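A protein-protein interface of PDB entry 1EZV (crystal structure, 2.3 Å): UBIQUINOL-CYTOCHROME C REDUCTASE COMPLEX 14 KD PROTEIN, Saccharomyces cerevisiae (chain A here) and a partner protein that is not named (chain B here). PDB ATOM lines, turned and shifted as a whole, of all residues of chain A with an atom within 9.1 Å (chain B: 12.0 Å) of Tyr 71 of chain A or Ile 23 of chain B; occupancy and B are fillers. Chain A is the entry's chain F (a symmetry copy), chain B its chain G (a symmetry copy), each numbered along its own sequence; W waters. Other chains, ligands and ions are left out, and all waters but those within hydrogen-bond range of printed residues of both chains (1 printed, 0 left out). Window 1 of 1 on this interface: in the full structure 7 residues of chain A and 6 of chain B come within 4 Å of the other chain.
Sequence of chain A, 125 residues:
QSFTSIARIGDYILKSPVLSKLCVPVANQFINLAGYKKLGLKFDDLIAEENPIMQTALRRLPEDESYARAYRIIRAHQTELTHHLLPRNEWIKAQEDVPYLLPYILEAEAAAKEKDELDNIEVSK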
ATOM      1  N   LEU A  39       7.013  18.182  10.059  1.00  0.00           N
ATOM      2  CA  LEU A  39       7.246  17.292   8.923  1.00  0.00           C
ATOM      3  C   LEU A  39       7.803  15.941   9.374  1.00  0.00           C
ATOM      4  O   LEU A  39       8.027  15.045   8.549  1.00  0.00           O
ATOM      5  CB  LEU A  39       8.232  17.935   7.943  1.00  0.00           C
ATOM      6  CG  LEU A  39       7.684  18.620   6.692  1.00  0.00           C
ATOM      7  CD1 LEU A  39       6.324  19.227   6.949  1.00  0.00           C
ATOM      8  CD2 LEU A  39       8.667  19.688   6.256  1.00  0.00           C
ATOM      9  N   GLY A  40       8.112  15.831  10.664  1.00  0.00           N
ATOM     10  CA  GLY A  40       8.591  14.575  11.205  1.00  0.00           C
ATOM     11  C   GLY A  40      10.100  14.471  11.189  1.00  0.00           C
ATOM     12  O   GLY A  40      10.654  13.378  11.297  1.00  0.00           O
ATOM     13  N   LEU A  41      10.765  15.614  11.093  1.00  0.00           N
ATOM     14  CA  LEU A  41      12.221  15.648  11.035  1.00  0.00           C
ATOM     15  C   LEU A  41      12.836  16.019  12.371  1.00  0.00           C
ATOM     16  O   LEU A  41      12.200  16.659  13.211  1.00  0.00           O
ATOM     17  CB  LEU A  41      12.698  16.642   9.965  1.00  0.00           C
ATOM     18  CG  LEU A  41      12.384  16.256   8.517  1.00  0.00           C
ATOM     19  CD1 LEU A  41      12.536  17.464   7.599  1.00  0.00           C
ATOM     20  CD2 LEU A  41      13.298  15.133   8.087  1.00  0.00           C
ATOM     21  N   ASP A  45      18.693  15.693  10.855  1.00  0.00           N
ATOM     22  CA  ASP A  45      18.289  15.236   9.517  1.00  0.00           C
ATOM     23  C   ASP A  45      18.453  16.330   8.462  1.00  0.00           C
ATOM     24  O   ASP A  45      18.467  16.044   7.272  1.00  0.00           O
ATOM     25  CB  ASP A  45      16.826  14.784   9.493  1.00  0.00           C
ATOM     26  CG  ASP A  45      16.511  13.718  10.522  1.00  0.00           C
ATOM     27  OD1 ASP A  45      17.385  12.900  10.853  1.00  0.00           O
ATOM     28  OD2 ASP A  45      15.347  13.648  10.944  1.00  0.00           O
ATOM     29  N   ASP A  64      20.497   1.101  13.013  1.00  0.00           N
ATOM     30  CA  ASP A  64      19.110   1.353  13.388  1.00  0.00           C
ATOM     31  C   ASP A  64      18.735   2.824  13.305  1.00  0.00           C
ATOM     32  O   ASP A  64      17.624   3.168  12.907  1.00  0.00           O
ATOM     33  CB  ASP A  64      18.838   0.813  14.793  1.00  0.00           C
ATOM     34  CG  ASP A  64      18.747  -0.701  14.817  1.00  0.00           C
ATOM     35  OD1 ASP A  64      17.920  -1.263  14.059  1.00  0.00           O
ATOM     36  OD2 ASP A  64      19.536  -1.331  15.559  1.00  0.00           O
ATOM     37  N   GLU A  65      19.687   3.688  13.640  1.00  0.00           N
ATOM     38  CA  GLU A  65      19.520   5.119  13.456  1.00  0.00           C
ATOM     39  C   GLU A  65      19.536   5.484  11.968  1.00  0.00           C
ATOM     40  O   GLU A  65      18.723   6.293  11.510  1.00  0.00           O
ATOM     41  CB  GLU A  65      20.627   5.866  14.200  1.00  0.00           C
ATOM     42  CG  GLU A  65      20.607   5.650  15.710  1.00  0.00           C
ATOM     43  CD  GLU A  65      20.140   6.877  16.470  1.00  0.00           C
ATOM     44  OE1 GLU A  65      20.985   7.503  17.150  1.00  0.00           O
ATOM     45  OE2 GLU A  65      18.941   7.229  16.366  1.00  0.00           O
ATOM     46  N   SER A  66      20.368   4.783  11.200  1.00  0.00           N
ATOM     47  CA  SER A  66      20.445   5.004   9.761  1.00  0.00           C
ATOM     48  C   SER A  66      19.133   4.707   9.038  1.00  0.00           C
ATOM     49  O   SER A  66      18.667   5.518   8.234  1.00  0.00           O
ATOM     50  CB  SER A  66      21.559   4.171   9.155  1.00  0.00           C
ATOM     51  OG  SER A  66      21.707   4.500   7.789  1.00  0.00           O
ATOM     52  N   TYR A  67      18.515   3.575   9.360  1.00  0.00           N
ATOM     53  CA  TYR A  67      17.231   3.216   8.756  1.00  0.00           C
ATOM     54  C   TYR A  67      16.150   4.206   9.179  1.00  0.00           C
ATOM     55  O   TYR A  67      15.239   4.510   8.407  1.00  0.00           O
ATOM     56  CB  TYR A  67      16.802   1.797   9.165  1.00  0.00           C
ATOM     57  CG  TYR A  67      17.755   0.687   8.763  1.00  0.00           C
ATOM     58  CD1 TYR A  67      17.969  -0.406   9.605  1.00  0.00           C
ATOM     59  CD2 TYR A  67      18.419   0.708   7.528  1.00  0.00           C
ATOM     60  CE1 TYR A  67      18.812  -1.449   9.229  1.00  0.00           C
ATOM     61  CE2 TYR A  67      19.267  -0.329   7.146  1.00  0.00           C
ATOM     62  CZ  TYR A  67      19.455  -1.407   8.001  1.00  0.00           C
ATOM     63  OH  TYR A  67      20.276  -2.449   7.628  1.00  0.00           O
ATOM     64  N   ALA A  68      16.257   4.704  10.410  1.00  0.00           N
ATOM     65  CA  ALA A  68      15.285   5.653  10.945  1.00  0.00           C
ATOM     66  C   ALA A  68      15.383   7.026  10.264  1.00  0.00           C
ATOM     67  O   ALA A  68      14.360   7.602   9.882  1.00  0.00           O
ATOM     68  CB  ALA A  68      15.465   5.792  12.460  1.00  0.00           C
ATOM     69  N   ARG A  69      16.611   7.524  10.088  1.00  0.00           N
ATOM     70  CA  ARG A  69      16.845   8.754   9.331  1.00  0.00           C
ATOM     71  C   ARG A  69      16.271   8.641   7.918  1.00  0.00           C
ATOM     72  O   ARG A  69      15.555   9.537   7.462  1.00  0.00           O
ATOM     73  CB  ARG A  69      18.347   9.100   9.257  1.00  0.00           C
ATOM     74  CG  ARG A  69      18.597  10.503   8.697  1.00  0.00           C
ATOM     75  CD  ARG A  69      20.070  10.871   8.556  1.00  0.00           C
ATOM     76  NE  ARG A  69      20.632  10.207   7.399  1.00  0.00           N
ATOM     77  CZ  ARG A  69      20.853  10.770   6.220  1.00  0.00           C
ATOM     78  NH1 ARG A  69      20.982   9.974   5.176  1.00  0.00           N
ATOM     79  NH2 ARG A  69      21.204  12.055   6.117  1.00  0.00           N
ATOM     80  N   ALA A  70      16.460   7.477   7.300  1.00  0.00           N
ATOM     81  CA  ALA A  70      15.988   7.230   5.937  1.00  0.00           C
ATOM     82  C   ALA A  70      14.468   7.333   5.839  1.00  0.00           C
ATOM     83  O   ALA A  70      13.935   7.973   4.926  1.00  0.00           O
ATOM     84  CB  ALA A  70      16.455   5.853   5.456  1.00  0.00           C
ATOM     85  N   TYR A  71      13.776   6.749   6.813  1.00  0.00           N
ATOM     86  CA  TYR A  71      12.319   6.829   6.867  1.00  0.00           C
ATOM     87  C   TYR A  71      11.829   8.258   7.098  1.00  0.00           C
ATOM     88  O   TYR A  71      10.857   8.689   6.476  1.00  0.00           O
ATOM     89  CB  TYR A  71      11.766   5.908   7.969  1.00  0.00           C
ATOM     90  CG  TYR A  71      10.265   5.979   8.113  1.00  0.00           C
ATOM     91  CD1 TYR A  71       9.432   5.649   7.046  1.00  0.00           C
ATOM     92  CD2 TYR A  71       9.677   6.486   9.274  1.00  0.00           C
ATOM     93  CE1 TYR A  71       8.050   5.830   7.123  1.00  0.00           C
ATOM     94  CE2 TYR A  71       8.292   6.677   9.360  1.00  0.00           C
ATOM     95  CZ  TYR A  71       7.488   6.345   8.280  1.00  0.00           C
ATOM     96  OH  TYR A  71       6.120   6.530   8.346  1.00  0.00           O
ATOM     97  N   ARG A  72      12.471   8.973   8.018  1.00  0.00           N
ATOM     98  CA  ARG A  72      12.049  10.331   8.349  1.00  0.00           C
ATOM     99  C   ARG A  72      12.211  11.268   7.157  1.00  0.00           C
ATOM    100  O   ARG A  72      11.315  12.062   6.856  1.00  0.00           O
ATOM    101  CB  ARG A  72      12.837  10.867   9.550  1.00  0.00           C
ATOM    102  CG  ARG A  72      12.449  10.242  10.881  1.00  0.00           C
ATOM    103  CD  ARG A  72      12.973  11.053  12.059  1.00  0.00           C
ATOM    104  NE  ARG A  72      14.427  11.233  12.026  1.00  0.00           N
ATOM    105  CZ  ARG A  72      15.311  10.386  12.546  1.00  0.00           C
ATOM    106  NH1 ARG A  72      16.609  10.645  12.454  1.00  0.00           N
ATOM    107  NH2 ARG A  72      14.906   9.270  13.133  1.00  0.00           N
ATOM    108  N   ILE A  73      13.301  11.088   6.416  1.00  0.00           N
ATOM    109  CA  ILE A  73      13.559  11.871   5.210  1.00  0.00           C
ATOM    110  C   ILE A  73      12.563  11.562   4.077  1.00  0.00           C
ATOM    111  O   ILE A  73      11.968  12.477   3.484  1.00  0.00           O
ATOM    112  CB  ILE A  73      15.011  11.651   4.731  1.00  0.00           C
ATOM    113  CG1 ILE A  73      15.976  12.303   5.732  1.00  0.00           C
ATOM    114  CG2 ILE A  73      15.213  12.245   3.332  1.00  0.00           C
ATOM    115  CD1 ILE A  73      17.438  11.973   5.501  1.00  0.00           C
ATOM    116  N   ILE A  74      12.301  10.280   3.849  1.00  0.00           N
ATOM    117  CA  ILE A  74      11.336   9.896   2.824  1.00  0.00           C
ATOM    118  C   ILE A  74       9.938  10.384   3.186  1.00  0.00           C
ATOM    119  O   ILE A  74       9.265  11.018   2.372  1.00  0.00           O
ATOM    120  CB  ILE A  74      11.321   8.371   2.602  1.00  0.00           C
ATOM    121  CG1 ILE A  74      12.654   7.926   2.000  1.00  0.00           C
ATOM    122  CG2 ILE A  74      10.188   7.986   1.676  1.00  0.00           C
ATOM    123  CD1 ILE A  74      12.804   6.425   1.873  1.00  0.00           C
ATOM    124  N   ARG A  75       9.571  10.229   4.451  1.00  0.00           N
ATOM    125  CA  ARG A  75       8.265  10.690   4.934  1.00  0.00           C
ATOM    126  C   ARG A  75       8.113  12.214   4.834  1.00  0.00           C
ATOM    127  O   ARG A  75       7.054  12.714   4.454  1.00  0.00           O
ATOM    128  CB  ARG A  75       8.055  10.218   6.379  1.00  0.00           C
ATOM    129  CG  ARG A  75       6.723  10.586   6.991  1.00  0.00           C
ATOM    130  CD  ARG A  75       6.951  11.191   8.362  1.00  0.00           C
ATOM    131  NE  ARG A  75       6.848  10.212   9.439  1.00  0.00           N
ATOM    132  CZ  ARG A  75       7.483  10.288  10.604  1.00  0.00           C
ATOM    133  NH1 ARG A  75       7.169   9.434  11.564  1.00  0.00           N
ATOM    134  NH2 ARG A  75       8.507  11.115  10.773  1.00  0.00           N
ATOM    135  N   ALA A  76       9.204  12.939   5.071  1.00  0.00           N
ATOM    136  CA  ALA A  76       9.201  14.392   4.913  1.00  0.00           C
ATOM    137  C   ALA A  76       8.977  14.831   3.456  1.00  0.00           C
ATOM    138  O   ALA A  76       8.199  15.758   3.198  1.00  0.00           O
ATOM    139  CB  ALA A  76      10.505  14.980   5.449  1.00  0.00           C
ATOM    140  N   HIS A  77       9.629  14.157   2.505  1.00  0.00           N
ATOM    141  CA  HIS A  77       9.449  14.494   1.092  1.00  0.00           C
ATOM    142  C   HIS A  77       8.030  14.244   0.606  1.00  0.00           C
ATOM    143  O   HIS A  77       7.455  15.089  -0.092  1.00  0.00           O
ATOM    144  CB  HIS A  77      10.440  13.727   0.212  1.00  0.00           C
ATOM    145  CG  HIS A  77      11.810  14.328   0.190  1.00  0.00           C
ATOM    146  ND1 HIS A  77      12.910  13.696   0.727  1.00  0.00           N
ATOM    147  CD2 HIS A  77      12.264  15.490  -0.337  1.00  0.00           C
ATOM    148  CE1 HIS A  77      13.986  14.433   0.520  1.00  0.00           C
ATOM    149  NE2 HIS A  77      13.620  15.527  -0.126  1.00  0.00           N
ATOM    150  N   GLN A  78       7.464  13.106   1.003  1.00  0.00           N
ATOM    151  CA  GLN A  78       6.094  12.757   0.643  1.00  0.00           C
ATOM    152  C   GLN A  78       5.079  13.742   1.211  1.00  0.00           C
ATOM    153  O   GLN A  78       4.136  14.135   0.521  1.00  0.00           O
ATOM    154  CB  GLN A  78       5.751  11.348   1.122  1.00  0.00           C
ATOM    155  CG  GLN A  78       4.322  10.932   0.797  1.00  0.00           C
ATOM    156  CD  GLN A  78       4.057  10.862  -0.699  1.00  0.00           C
ATOM    157  OE1 GLN A  78       4.947  10.527  -1.485  1.00  0.00           O
ATOM    158  NE2 GLN A  78       2.835  11.185  -1.101  1.00  0.00           N
ATOM    159  N   THR A  79       5.278  14.162   2.458  1.00  0.00           N
ATOM    160  CA  THR A  79       4.373  15.136   3.056  1.00  0.00           C
ATOM    161  C   THR A  79       4.538  16.508   2.403  1.00  0.00           C
ATOM    162  O   THR A  79       3.554  17.167   2.073  1.00  0.00           O
ATOM    163  CB  THR A  79       4.599  15.260   4.581  1.00  0.00           C
ATOM    164  OG1 THR A  79       4.710  13.953   5.153  1.00  0.00           O
ATOM    165  CG2 THR A  79       3.428  15.981   5.230  1.00  0.00           C
ATOM    166  N   LEU A  86       2.161  16.570   8.876  1.00  0.00           N
ATOM    167  CA  LEU A  86       1.728  15.321   9.474  1.00  0.00           C
ATOM    168  C   LEU A  86       0.628  15.596  10.505  1.00  0.00           C
ATOM    169  O   LEU A  86       0.475  16.724  10.972  1.00  0.00           O
ATOM    170  CB  LEU A  86       2.919  14.627  10.130  1.00  0.00           C
ATOM    171  CG  LEU A  86       4.020  14.165   9.172  1.00  0.00           C
ATOM    172  CD1 LEU A  86       5.207  13.650   9.972  1.00  0.00           C
ATOM    173  CD2 LEU A  86       3.482  13.080   8.249  1.00  0.00           C
ATOM    174  N   GLU A  90       2.061  12.681  15.216  1.00  0.00           N
ATOM    175  CA  GLU A  90       3.225  12.143  14.519  1.00  0.00           C
ATOM    176  C   GLU A  90       4.421  13.097  14.521  1.00  0.00           C
ATOM    177  O   GLU A  90       5.517  12.716  14.107  1.00  0.00           O
ATOM    178  CB  GLU A  90       2.864  11.792  13.075  1.00  0.00           C
ATOM    179  CG  GLU A  90       2.189  10.443  12.891  1.00  0.00           C
ATOM    180  CD  GLU A  90       1.869  10.161  11.435  1.00  0.00           C
ATOM    181  OE1 GLU A  90       2.810   9.859  10.664  1.00  0.00           O
ATOM    182  OE2 GLU A  90       0.683  10.278  11.054  1.00  0.00           O
ATOM    183  N   ILE A  92       7.631  15.296  15.639  1.00  0.00           N
ATOM    184  CA  ILE A  92       8.751  15.002  16.519  1.00  0.00           C
ATOM    185  C   ILE A  92       8.615  15.850  17.779  1.00  0.00           C
ATOM    186  O   ILE A  92       8.330  17.045  17.708  1.00  0.00           O
ATOM    187  CB  ILE A  92      10.105  15.297  15.824  1.00  0.00           C
ATOM    188  CG1 ILE A  92      10.330  14.309  14.675  1.00  0.00           C
ATOM    189  CG2 ILE A  92      11.256  15.219  16.823  1.00  0.00           C
ATOM    190  CD1 ILE A  92      10.267  12.848  15.075  1.00  0.00           C
ATOM    191  N   GLY B  17      22.142   6.880  -2.116  1.00  0.00           N
ATOM    192  CA  GLY B  17      21.519   6.972  -0.811  1.00  0.00           C
ATOM    193  C   GLY B  17      22.041   5.917   0.146  1.00  0.00           C
ATOM    194  O   GLY B  17      22.817   5.038  -0.251  1.00  0.00           O
ATOM    195  N   PRO B  18      21.633   5.975   1.422  1.00  0.00           N
ATOM    196  CA  PRO B  18      21.935   4.912   2.388  1.00  0.00           C
ATOM    197  C   PRO B  18      21.106   3.667   2.079  1.00  0.00           C
ATOM    198  O   PRO B  18      20.062   3.763   1.426  1.00  0.00           O
ATOM    199  CB  PRO B  18      21.529   5.534   3.723  1.00  0.00           C
ATOM    200  CG  PRO B  18      20.361   6.408   3.356  1.00  0.00           C
ATOM    201  CD  PRO B  18      20.769   7.014   2.015  1.00  0.00           C
ATOM    202  N   LYS B  19      21.536   2.522   2.604  1.00  0.00           N
ATOM    203  CA  LYS B  19      20.785   1.274   2.455  1.00  0.00           C
ATOM    204  C   LYS B  19      19.425   1.367   3.148  1.00  0.00           C
ATOM    205  O   LYS B  19      19.339   1.789   4.292  1.00  0.00           O
ATOM    206  CB  LYS B  19      21.581   0.102   3.035  1.00  0.00           C
ATOM    207  CG  LYS B  19      23.003  -0.012   2.509  1.00  0.00           C
ATOM    208  CD  LYS B  19      23.298  -1.402   1.979  1.00  0.00           C
ATOM    209  CE  LYS B  19      24.772  -1.552   1.591  1.00  0.00           C
ATOM    210  NZ  LYS B  19      25.211  -0.569   0.539  1.00  0.00           N
ATOM    211  N   GLN B  20      18.360   1.057   2.422  1.00  0.00           N
ATOM    212  CA  GLN B  20      17.008   1.175   2.959  1.00  0.00           C
ATOM    213  C   GLN B  20      16.483  -0.196   3.342  1.00  0.00           C
ATOM    214  O   GLN B  20      16.595  -1.146   2.572  1.00  0.00           O
ATOM    215  CB  GLN B  20      16.064   1.814   1.927  1.00  0.00           C
ATOM    216  CG  GLN B  20      16.323   3.293   1.652  1.00  0.00           C
ATOM    217  CD  GLN B  20      15.332   3.884   0.663  1.00  0.00           C
ATOM    218  OE1 GLN B  20      14.180   3.460   0.596  1.00  0.00           O
ATOM    219  NE2 GLN B  20      15.779   4.863  -0.119  1.00  0.00           N
ATOM    220  N   LYS B  21      15.928  -0.295   4.545  1.00  0.00           N
ATOM    221  CA  LYS B  21      15.356  -1.539   5.048  1.00  0.00           C
ATOM    222  C   LYS B  21      14.229  -1.182   6.010  1.00  0.00           C
ATOM    223  O   LYS B  21      14.332  -0.205   6.749  1.00  0.00           O
ATOM    224  CB  LYS B  21      16.428  -2.344   5.784  1.00  0.00           C
ATOM    225  CG  LYS B  21      16.011  -3.757   6.187  1.00  0.00           C
ATOM    226  CD  LYS B  21      17.139  -4.444   6.967  1.00  0.00           C
ATOM    227  CE  LYS B  21      17.098  -5.960   6.833  1.00  0.00           C
ATOM    228  NZ  LYS B  21      15.783  -6.511   7.236  1.00  0.00           N
ATOM    229  N   GLY B  22      13.121  -1.912   5.928  1.00  0.00           N
ATOM    230  CA  GLY B  22      12.032  -1.711   6.864  1.00  0.00           C
ATOM    231  C   GLY B  22      10.917  -0.809   6.374  1.00  0.00           C
ATOM    232  O   GLY B  22       9.829  -0.789   6.961  1.00  0.00           O
ATOM    233  N   ILE B  23      11.200   0.000   5.356  1.00  0.00           N
ATOM    234  CA  ILE B  23      10.190   0.891   4.781  1.00  0.00           C
ATOM    235  C   ILE B  23       9.422   0.158   3.681  1.00  0.00           C
ATOM    236  O   ILE B  23      10.022  -0.425   2.780  1.00  0.00           O
ATOM    237  CB  ILE B  23      10.841   2.160   4.183  1.00  0.00           C
ATOM    238  CG1 ILE B  23      11.680   2.867   5.251  1.00  0.00           C
ATOM    239  CG2 ILE B  23       9.768   3.095   3.624  1.00  0.00           C
ATOM    240  CD1 ILE B  23      12.801   3.728   4.699  1.00  0.00           C
ATOM    241  N   THR B  24       8.098   0.184   3.772  1.00  0.00           N
ATOM    242  CA  THR B  24       7.231  -0.455   2.792  1.00  0.00           C
ATOM    243  C   THR B  24       6.273   0.598   2.246  1.00  0.00           C
ATOM    244  O   THR B  24       5.622   1.301   3.019  1.00  0.00           O
ATOM    245  CB  THR B  24       6.413  -1.598   3.456  1.00  0.00           C
ATOM    246  OG1 THR B  24       7.312  -2.610   3.919  1.00  0.00           O
ATOM    247  CG2 THR B  24       5.422  -2.218   2.481  1.00  0.00           C
ATOM    248  N   SER B  25       6.185   0.718   0.922  1.00  0.00           N
ATOM    249  CA  SER B  25       5.306   1.723   0.335  1.00  0.00           C
ATOM    250  C   SER B  25       4.145   1.098  -0.408  1.00  0.00           C
ATOM    251  O   SER B  25       4.229  -0.035  -0.871  1.00  0.00           O
ATOM    252  CB  SER B  25       6.087   2.652  -0.598  1.00  0.00           C
ATOM    253  OG  SER B  25       6.518   1.968  -1.759  1.00  0.00           O
ATOM    254  N   TYR B  26       3.050   1.840  -0.500  1.00  0.00           N
ATOM    255  CA  TYR B  26       1.847   1.355  -1.164  1.00  0.00           C
ATOM    256  C   TYR B  26       1.326   2.456  -2.071  1.00  0.00           C
ATOM    257  O   TYR B  26       1.392   3.632  -1.712  1.00  0.00           O
ATOM    258  CB  TYR B  26       0.761   1.005  -0.137  1.00  0.00           C
ATOM    259  CG  TYR B  26       1.163  -0.034   0.887  1.00  0.00           C
ATOM    260  CD1 TYR B  26       1.865   0.328   2.037  1.00  0.00           C
ATOM    261  CD2 TYR B  26       0.764  -1.366   0.752  1.00  0.00           C
ATOM    262  CE1 TYR B  26       2.156  -0.604   3.023  1.00  0.00           C
ATOM    263  CE2 TYR B  26       1.037  -2.306   1.745  1.00  0.00           C
ATOM    264  CZ  TYR B  26       1.733  -1.918   2.875  1.00  0.00           C
ATOM    265  OH  TYR B  26       2.002  -2.835   3.869  1.00  0.00           O
ATOM    266  N   ALA B  27       0.737   2.073  -3.200  1.00  0.00           N
ATOM    267  CA  ALA B  27       0.083   3.040  -4.067  1.00  0.00           C
ATOM    268  C   ALA B  27      -1.026   2.378  -4.878  1.00  0.00           C
ATOM    269  O   ALA B  27      -1.075   1.156  -4.995  1.00  0.00           O
ATOM    270  CB  ALA B  27       1.116   3.699  -5.004  1.00  0.00           C
HETATM  271  O   HOH W   1      21.309   2.544   5.909  1.00  0.00           O
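Water W1 lies within hydrogen-bond range of O of Lys 19 of chain B (2.7 Å) and OG of Ser 66 of chain A (2.7 Å).
Among the printed residues, pairs that only touch across the chains: Tyr 67 of chain A with Lys 19 of chain B, Tyr 67 of chain A with Lys 21 of chain B, Tyr 71 of chain A with Ile 23 of chain B, Ile 74 of chain A with Gln 20 of chain B and Ile 74 of chain A with Ile 23 of chain B.
Of the 23 printed residues of chain A, 3 touch a printed residue of chain B.
Hydrophobic or aromatic side chains of chain A that line the printed part of chain B: Tyr 67 and Ile 74.
Among the printed residues, 5 pairs touch across the chains.
Among the printed residues, no Asp or Glu carboxylate lies within 4 Å of a Lys or Arg side-chain nitrogen of the other chain.
Of the printed residues of chain B, Tyr 71 of chain A touches Ile 23 (3.8 Å).
No residue of chain B comes within 4 Å of Ala 68 of chain A.
No residue of chain B comes within 4 Å of Ala 70 of chain A.
No residue of chain B comes within 4 Å of Ile 73 of chain A.
Ile 74 of chain A touches two residues of chain B.
No residue of chain B comes within 4 Å of Arg 75 of chain A.
Gly 22 of chain B touches none of the printed residues of chain A.
No residue of chain A comes within 4 Å of Thr 24 of chain B.
Printed residues of chain A within 4 Å of Lys 19 of chain B: Tyr 67.
Of the printed residues of chain B, Tyr 67 of chain A touches Lys 19 and Lys 21.
Of the printed residues of chain A, Gln 20 of chain B touches Ile 74 (3.5 Å).
Printed residues of chain A within 4 Å of Lys 21 of chain B: Tyr 67.
The nearest residue of chain B that does not touch Tyr 71 of chain A is Gly 22 of chain B (6.5 Å).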
